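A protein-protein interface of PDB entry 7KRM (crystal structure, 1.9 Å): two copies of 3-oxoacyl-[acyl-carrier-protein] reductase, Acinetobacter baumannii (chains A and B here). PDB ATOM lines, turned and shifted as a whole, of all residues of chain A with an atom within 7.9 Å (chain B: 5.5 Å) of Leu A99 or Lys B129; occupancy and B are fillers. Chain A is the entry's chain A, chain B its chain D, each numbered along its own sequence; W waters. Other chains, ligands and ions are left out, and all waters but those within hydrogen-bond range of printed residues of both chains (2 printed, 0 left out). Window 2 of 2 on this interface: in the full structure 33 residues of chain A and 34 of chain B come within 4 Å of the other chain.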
ATOM      1  N   ILE A  96       8.840  -4.511 -23.483  1.00  0.00           N
ATOM      2  CA  ILE A  96       8.276  -3.860 -24.658  1.00  0.00           C
ATOM      3  C   ILE A  96       6.786  -4.160 -24.710  1.00  0.00           C
ATOM      4  O   ILE A  96       6.331  -5.229 -24.290  1.00  0.00           O
ATOM      5  CB  ILE A  96       8.968  -4.305 -25.966  1.00  0.00           C
ATOM      6  CG1 ILE A  96       8.847  -5.817 -26.154  1.00  0.00           C
ATOM      7  CG2 ILE A  96      10.433  -3.887 -25.957  1.00  0.00           C
ATOM      8  CD1 ILE A  96       9.478  -6.320 -27.436  1.00  0.00           C
ATOM      9  N   LYS A  97       6.025  -3.207 -25.237  1.00  0.00           N
ATOM     10  CA  LYS A  97       4.577  -3.313 -25.276  1.00  0.00           C
ATOM     11  C   LYS A  97       4.120  -4.066 -26.523  1.00  0.00           C
ATOM     12  O   LYS A  97       4.887  -4.300 -27.459  1.00  0.00           O
ATOM     13  CB  LYS A  97       3.942  -1.924 -25.231  1.00  0.00           C
ATOM     14  CG  LYS A  97       4.234  -1.151 -23.954  1.00  0.00           C
ATOM     15  CD  LYS A  97       3.349   0.085 -23.841  1.00  0.00           C
ATOM     16  CE  LYS A  97       3.716   1.145 -24.871  1.00  0.00           C
ATOM     17  NZ  LYS A  97       2.621   2.138 -25.066  1.00  0.00           N
ATOM     18  N   THR A  98       2.831  -4.423 -26.528  1.00  0.00           N
ATOM     19  CA  THR A  98       2.274  -5.293 -27.560  1.00  0.00           C
ATOM     20  C   THR A  98       2.661  -4.842 -28.964  1.00  0.00           C
ATOM     21  O   THR A  98       3.181  -5.631 -29.761  1.00  0.00           O
ATOM     22  CB  THR A  98       0.747  -5.338 -27.434  1.00  0.00           C
ATOM     23  OG1 THR A  98       0.379  -5.850 -26.149  1.00  0.00           O
ATOM     24  CG2 THR A  98       0.140  -6.218 -28.521  1.00  0.00           C
ATOM     25  N   LEU A  99       2.389  -3.579 -29.296  1.00  0.00           N
ATOM     26  CA  LEU A  99       2.559  -3.110 -30.666  1.00  0.00           C
ATOM     27  C   LEU A  99       4.020  -2.960 -31.072  1.00  0.00           C
ATOM     28  O   LEU A  99       4.291  -2.766 -32.262  1.00  0.00           O
ATOM     29  CB  LEU A  99       1.835  -1.773 -30.851  1.00  0.00           C
ATOM     30  CG  LEU A  99       0.329  -1.786 -30.581  1.00  0.00           C
ATOM     31  CD1 LEU A  99      -0.266  -0.397 -30.775  1.00  0.00           C
ATOM     32  CD2 LEU A  99      -0.374  -2.799 -31.471  1.00  0.00           C
ATOM     33  N   ASP A 100       4.957  -3.051 -30.130  1.00  0.00           N
ATOM     34  CA  ASP A 100       6.376  -2.912 -30.428  1.00  0.00           C
ATOM     35  C   ASP A 100       7.099  -4.249 -30.532  1.00  0.00           C
ATOM     36  O   ASP A 100       8.302  -4.266 -30.806  1.00  0.00           O
ATOM     37  CB  ASP A 100       7.053  -2.050 -29.358  1.00  0.00           C
ATOM     38  CG  ASP A 100       6.463  -0.659 -29.275  1.00  0.00           C
ATOM     39  OD1 ASP A 100       6.123  -0.094 -30.336  1.00  0.00           O
ATOM     40  OD2 ASP A 100       6.333  -0.134 -28.149  1.00  0.00           O
ATOM     41  N   ILE A 101       6.401  -5.362 -30.314  1.00  0.00           N
ATOM     42  CA  ILE A 101       7.033  -6.677 -30.380  1.00  0.00           C
ATOM     43  C   ILE A 101       7.305  -7.021 -31.839  1.00  0.00           C
ATOM     44  O   ILE A 101       6.377  -7.133 -32.649  1.00  0.00           O
ATOM     45  CB  ILE A 101       6.152  -7.744 -29.718  1.00  0.00           C
ATOM     46  CG1 ILE A 101       5.934  -7.421 -28.239  1.00  0.00           C
ATOM     47  CG2 ILE A 101       6.786  -9.122 -29.873  1.00  0.00           C
ATOM     48  CD1 ILE A 101       4.853  -8.258 -27.587  1.00  0.00           C
ATOM     49  N   GLN A 102       8.578  -7.194 -32.177  1.00  0.00           N
ATOM     50  CA  GLN A 102       8.985  -7.598 -33.513  1.00  0.00           C
ATOM     51  C   GLN A 102       9.237  -9.102 -33.547  1.00  0.00           C
ATOM     52  O   GLN A 102       9.324  -9.769 -32.514  1.00  0.00           O
ATOM     53  CB  GLN A 102      10.240  -6.835 -33.948  1.00  0.00           C
ATOM     54  CG  GLN A 102      10.092  -5.323 -33.889  1.00  0.00           C
ATOM     55  CD  GLN A 102      11.375  -4.600 -34.251  1.00  0.00           C
ATOM     56  OE1 GLN A 102      12.004  -3.965 -33.404  1.00  0.00           O
ATOM     57  NE2 GLN A 102      11.769  -4.691 -35.516  1.00  0.00           N
ATOM     58  N   PRO A 154       4.111  -8.608 -23.286  1.00  0.00           N
ATOM     59  CA  PRO A 154       3.148  -9.686 -23.576  1.00  0.00           C
ATOM     60  C   PRO A 154       3.780 -10.951 -24.133  1.00  0.00           C
ATOM     61  O   PRO A 154       3.274 -12.049 -23.872  1.00  0.00           O
ATOM     62  CB  PRO A 154       2.199  -9.040 -24.596  1.00  0.00           C
ATOM     63  CG  PRO A 154       2.291  -7.579 -24.327  1.00  0.00           C
ATOM     64  CD  PRO A 154       3.700  -7.321 -23.875  1.00  0.00           C
ATOM     65  N   SER B 121      -3.647  -9.383 -33.878  1.00  0.00           N
ATOM     66  CA  SER B 121      -4.037  -8.401 -32.873  1.00  0.00           C
ATOM     67  C   SER B 121      -3.281  -7.094 -33.071  1.00  0.00           C
ATOM     68  O   SER B 121      -3.871  -6.008 -33.035  1.00  0.00           O
ATOM     69  CB  SER B 121      -3.793  -8.964 -31.472  1.00  0.00           C
ATOM     70  OG  SER B 121      -4.622 -10.088 -31.222  1.00  0.00           O
ATOM     71  N   GLN B 122      -1.966  -7.181 -33.292  1.00  0.00           N
ATOM     72  CA  GLN B 122      -1.179  -5.981 -33.552  1.00  0.00           C
ATOM     73  C   GLN B 122      -1.755  -5.179 -34.713  1.00  0.00           C
ATOM     74  O   GLN B 122      -1.735  -3.945 -34.696  1.00  0.00           O
ATOM     75  CB  GLN B 122       0.274  -6.355 -33.844  1.00  0.00           C
ATOM     76  CG  GLN B 122       1.086  -6.765 -32.631  1.00  0.00           C
ATOM     77  CD  GLN B 122       2.482  -7.232 -33.006  1.00  0.00           C
ATOM     78  OE1 GLN B 122       2.670  -7.890 -34.027  1.00  0.00           O
ATOM     79  NE2 GLN B 122       3.465  -6.890 -32.185  1.00  0.00           N
ATOM     80  N   VAL B 124      -4.910  -5.002 -35.809  1.00  0.00           N
ATOM     81  CA  VAL B 124      -6.276  -4.514 -35.654  1.00  0.00           C
ATOM     82  C   VAL B 124      -6.378  -3.550 -34.478  1.00  0.00           C
ATOM     83  O   VAL B 124      -7.252  -2.675 -34.456  1.00  0.00           O
ATOM     84  CB  VAL B 124      -7.258  -5.690 -35.481  1.00  0.00           C
ATOM     85  CG1 VAL B 124      -8.659  -5.181 -35.194  1.00  0.00           C
ATOM     86  CG2 VAL B 124      -7.256  -6.571 -36.724  1.00  0.00           C
ATOM     87  N   ILE B 125      -5.490  -3.698 -33.491  1.00  0.00           N
ATOM     88  CA  ILE B 125      -5.587  -2.877 -32.280  1.00  0.00           C
ATOM     89  C   ILE B 125      -5.506  -1.392 -32.601  1.00  0.00           C
ATOM     90  O   ILE B 125      -6.282  -0.615 -32.025  1.00  0.00           O
ATOM     91  CB  ILE B 125      -4.542  -3.327 -31.250  1.00  0.00           C
ATOM     92  CG1 ILE B 125      -5.007  -4.610 -30.554  1.00  0.00           C
ATOM     93  CG2 ILE B 125      -4.286  -2.223 -30.223  1.00  0.00           C
ATOM     94  CD1 ILE B 125      -3.921  -5.298 -29.746  1.00  0.00           C
ATOM     95  N   PRO B 126      -4.611  -0.920 -33.474  1.00  0.00           N
ATOM     96  CA  PRO B 126      -4.557   0.530 -33.738  1.00  0.00           C
ATOM     97  C   PRO B 126      -5.896   1.122 -34.148  1.00  0.00           C
ATOM     98  O   PRO B 126      -6.269   2.193 -33.654  1.00  0.00           O
ATOM     99  CB  PRO B 126      -3.513   0.637 -34.858  1.00  0.00           C
ATOM    100  CG  PRO B 126      -2.640  -0.555 -34.672  1.00  0.00           C
ATOM    101  CD  PRO B 126      -3.549  -1.651 -34.189  1.00  0.00           C
ATOM    102  N   SER B 127      -6.635   0.449 -35.034  1.00  0.00           N
ATOM    103  CA  SER B 127      -7.946   0.949 -35.435  1.00  0.00           C
ATOM    104  C   SER B 127      -8.941   0.886 -34.282  1.00  0.00           C
ATOM    105  O   SER B 127      -9.754   1.800 -34.106  1.00  0.00           O
ATOM    106  CB  SER B 127      -8.468   0.156 -36.633  1.00  0.00           C
ATOM    107  OG  SER B 127      -8.823  -1.163 -36.257  1.00  0.00           O
ATOM    108  N   MET B 128      -8.905  -0.191 -33.492  1.00  0.00           N
ATOM    109  CA  MET B 128      -9.802  -0.293 -32.346  1.00  0.00           C
ATOM    110  C   MET B 128      -9.554   0.834 -31.351  1.00  0.00           C
ATOM    111  O   MET B 128     -10.503   1.434 -30.832  1.00  0.00           O
ATOM    112  CB  MET B 128      -9.627  -1.647 -31.658  1.00  0.00           C
ATOM    113  CG  MET B 128     -10.234  -2.812 -32.409  1.00  0.00           C
ATOM    114  SD  MET B 128     -10.019  -4.362 -31.510  1.00  0.00           S
ATOM    115  CE  MET B 128     -11.038  -5.465 -32.486  1.00  0.00           C
ATOM    116  N   LYS B 129      -8.285   1.124 -31.060  1.00  0.00           N
ATOM    117  CA  LYS B 129      -7.968   2.197 -30.125  1.00  0.00           C
ATOM    118  C   LYS B 129      -8.457   3.540 -30.651  1.00  0.00           C
ATOM    119  O   LYS B 129      -8.948   4.376 -29.882  1.00  0.00           O
ATOM    120  CB  LYS B 129      -6.461   2.223 -29.866  1.00  0.00           C
ATOM    121  CG  LYS B 129      -5.982   3.371 -28.990  1.00  0.00           C
ATOM    122  CD  LYS B 129      -4.602   3.092 -28.401  1.00  0.00           C
ATOM    123  CE  LYS B 129      -3.604   2.642 -29.460  1.00  0.00           C
ATOM    124  NZ  LYS B 129      -2.213   2.558 -28.928  1.00  0.00           N
ATOM    125  N   ALA B 130      -8.353   3.757 -31.963  1.00  0.00           N
ATOM    126  CA  ALA B 130      -8.805   5.016 -32.543  1.00  0.00           C
ATOM    127  C   ALA B 130     -10.325   5.107 -32.582  1.00  0.00           C
ATOM    128  O   ALA B 130     -10.880   6.206 -32.464  1.00  0.00           O
ATOM    129  CB  ALA B 130      -8.234   5.182 -33.953  1.00  0.00           C
ATOM    130  N   ASN B 131     -11.011   3.978 -32.745  1.00  0.00           N
ATOM    131  CA  ASN B 131     -12.464   3.959 -32.848  1.00  0.00           C
ATOM    132  C   ASN B 131     -13.156   3.813 -31.496  1.00  0.00           C
ATOM    133  O   ASN B 131     -14.379   3.645 -31.456  1.00  0.00           O
ATOM    134  CB  ASN B 131     -12.910   2.833 -33.783  1.00  0.00           C
ATOM    135  CG  ASN B 131     -12.493   3.071 -35.223  1.00  0.00           C
ATOM    136  OD1 ASN B 131     -11.834   2.232 -35.837  1.00  0.00           O
ATOM    137  ND2 ASN B 131     -12.874   4.221 -35.767  1.00  0.00           N
ATOM    138  N   GLY B 132     -12.411   3.866 -30.397  1.00  0.00           N
ATOM    139  CA  GLY B 132     -13.006   3.896 -29.078  1.00  0.00           C
ATOM    140  C   GLY B 132     -13.151   2.564 -28.381  1.00  0.00           C
ATOM    141  O   GLY B 132     -13.793   2.512 -27.325  1.00  0.00           O
ATOM    142  N   GLY B 133     -12.592   1.491 -28.928  1.00  0.00           N
ATOM    143  CA  GLY B 133     -12.596   0.210 -28.261  1.00  0.00           C
ATOM    144  C   GLY B 133     -12.937  -0.910 -29.220  1.00  0.00           C
ATOM    145  O   GLY B 133     -13.082  -0.710 -30.426  1.00  0.00           O
ATOM    146  N   GLU B 173      -3.082  -4.407 -20.878  1.00  0.00           N
ATOM    147  CA  GLU B 173      -2.467  -3.243 -21.507  1.00  0.00           C
ATOM    148  C   GLU B 173      -3.514  -2.312 -22.106  1.00  0.00           C
ATOM    149  O   GLU B 173      -3.382  -1.085 -22.017  1.00  0.00           O
ATOM    150  CB  GLU B 173      -1.471  -3.669 -22.590  1.00  0.00           C
ATOM    151  CG  GLU B 173      -0.925  -2.478 -23.379  1.00  0.00           C
ATOM    152  CD  GLU B 173       0.186  -2.833 -24.346  1.00  0.00           C
ATOM    153  OE1 GLU B 173       0.709  -3.966 -24.294  1.00  0.00           O
ATOM    154  OE2 GLU B 173       0.541  -1.960 -25.165  1.00  0.00           O
ATOM    155  N   PHE B 174      -4.552  -2.867 -22.732  1.00  0.00           N
ATOM    156  CA  PHE B 174      -5.496  -2.068 -23.504  1.00  0.00           C
ATOM    157  C   PHE B 174      -6.856  -1.927 -22.831  1.00  0.00           C
ATOM    158  O   PHE B 174      -7.813  -1.494 -23.480  1.00  0.00           O
ATOM    159  CB  PHE B 174      -5.656  -2.664 -24.903  1.00  0.00           C
ATOM    160  CG  PHE B 174      -4.382  -2.675 -25.698  1.00  0.00           C
ATOM    161  CD1 PHE B 174      -3.881  -1.502 -26.242  1.00  0.00           C
ATOM    162  CD2 PHE B 174      -3.678  -3.850 -25.892  1.00  0.00           C
ATOM    163  CE1 PHE B 174      -2.703  -1.503 -26.970  1.00  0.00           C
ATOM    164  CE2 PHE B 174      -2.500  -3.859 -26.619  1.00  0.00           C
ATOM    165  CZ  PHE B 174      -2.012  -2.683 -27.158  1.00  0.00           C
ATOM    166  N   ASP B 177      -8.168   1.505 -23.056  1.00  0.00           N
ATOM    167  CA  ASP B 177      -8.648   1.825 -24.393  1.00  0.00           C
ATOM    168  C   ASP B 177      -9.971   1.141 -24.715  1.00  0.00           C
ATOM    169  O   ASP B 177     -10.448   1.245 -25.849  1.00  0.00           O
ATOM    170  CB  ASP B 177      -7.591   1.436 -25.430  1.00  0.00           C
ATOM    171  CG  ASP B 177      -6.279   2.163 -25.220  1.00  0.00           C
ATOM    172  OD1 ASP B 177      -6.310   3.389 -24.993  1.00  0.00           O
ATOM    173  OD2 ASP B 177      -5.216   1.507 -25.268  1.00  0.00           O
ATOM    174  N   ILE B 179     -10.563  -1.923 -25.139  1.00  0.00           N
ATOM    175  CA  ILE B 179     -10.356  -3.075 -26.008  1.00  0.00           C
ATOM    176  C   ILE B 179     -10.367  -4.299 -25.100  1.00  0.00           C
ATOM    177  O   ILE B 179      -9.385  -4.587 -24.409  1.00  0.00           O
ATOM    178  CB  ILE B 179      -9.057  -2.966 -26.808  1.00  0.00           C
ATOM    179  CG1 ILE B 179      -9.070  -1.693 -27.657  1.00  0.00           C
ATOM    180  CG2 ILE B 179      -8.879  -4.192 -27.695  1.00  0.00           C
ATOM    181  CD1 ILE B 179      -7.781  -1.434 -28.405  1.00  0.00           C
HETATM  182  O   HOH W   1      -0.174   0.625 -24.797  1.00  0.00           O
HETATM  183  O   HOH W   2       1.519  -1.453 -27.504  1.00  0.00           O
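The side-chain amide nitrogen (NE2) of Gln B122 lies within hydrogen-bond range of the backbone carbonyl oxygen (O) of Ile A101 (3.0 Å). The backbone carbonyl oxygen (O) of Thr A98 is in hydrogen-bond range of the side-chain amide nitrogen (NE2) of Gln B122 (2.7 Å). The side-chain carboxylate (OE1) of Glu B173 lies within hydrogen-bond range of the side-chain hydroxyl (OG1) of Thr A98, at 2.7 Å.
The backbone carbonyl oxygen (O) of Phe B174 lies within hydrogen-bond range of the backbone NH (N) of Ile B179 (3.2 Å).
Lys A97 touches Glu B173 (CB to OE2, 3.4 Å). Thr A98 touches Phe B174 (OG1 to CE2, 3.5 Å). CD2 of Leu A99 touches O of Gln B122 (3.7 Å). CD1 of Leu A99 touches NZ of Lys B129, 3.99 Å away. Pro A154 touches Glu B173.
Ile A96 touches none of the printed residues of chain B. Printed residues of chain B within 4 Å of Lys A97: Glu B173. Of the printed residues of chain B, Leu A99 touches Gln B122 (3.7 Å) and Lys B129 (3.99 Å). Of the printed residues of chain B, Ile A101 touches Gln B122 (3.0 Å). Printed residues of chain B within 4 Å of Pro A154: Glu B173. Pro B126 touches none of the printed residues of chain A. Of the printed residues of chain A, Lys B129 touches Leu A99. Of the printed residues of chain A, Phe B174 touches Thr A98. The nearest printed residue of chain A that does not touch Lys B129 is Lys A97 (6.2 Å). The nearest printed residue of chain B that does not touch Thr A98 is Ile B125 (4.3 Å).
Of the 16 printed residues of chain B, 4 touch a printed residue of chain A. Hydrophobic or aromatic side chains of chain B within 4 Å of the printed part of chain A: Phe B174. Of the 8 printed residues of chain A, 5 touch a printed residue of chain B. Among the printed residues, 8 pairs touch across the chains. Among the printed residues, no Asp or Glu carboxylate lies within 4 Å of a Lys or Arg side-chain nitrogen of the other chain.
No position is printed for both chains.
Water W2 lies within hydrogen-bond range of the side-chain carboxylate (OE2) of Glu B173 (2.6 Å), the backbone NH (N) of Leu A99 (2.9 Å) and the backbone NH (N) of Thr A98 (3.4 Å). Water W1 lies within hydrogen-bond range of OE2 of Glu B173 (2.7 Å) and NZ of Lys A97 (3.2 Å).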
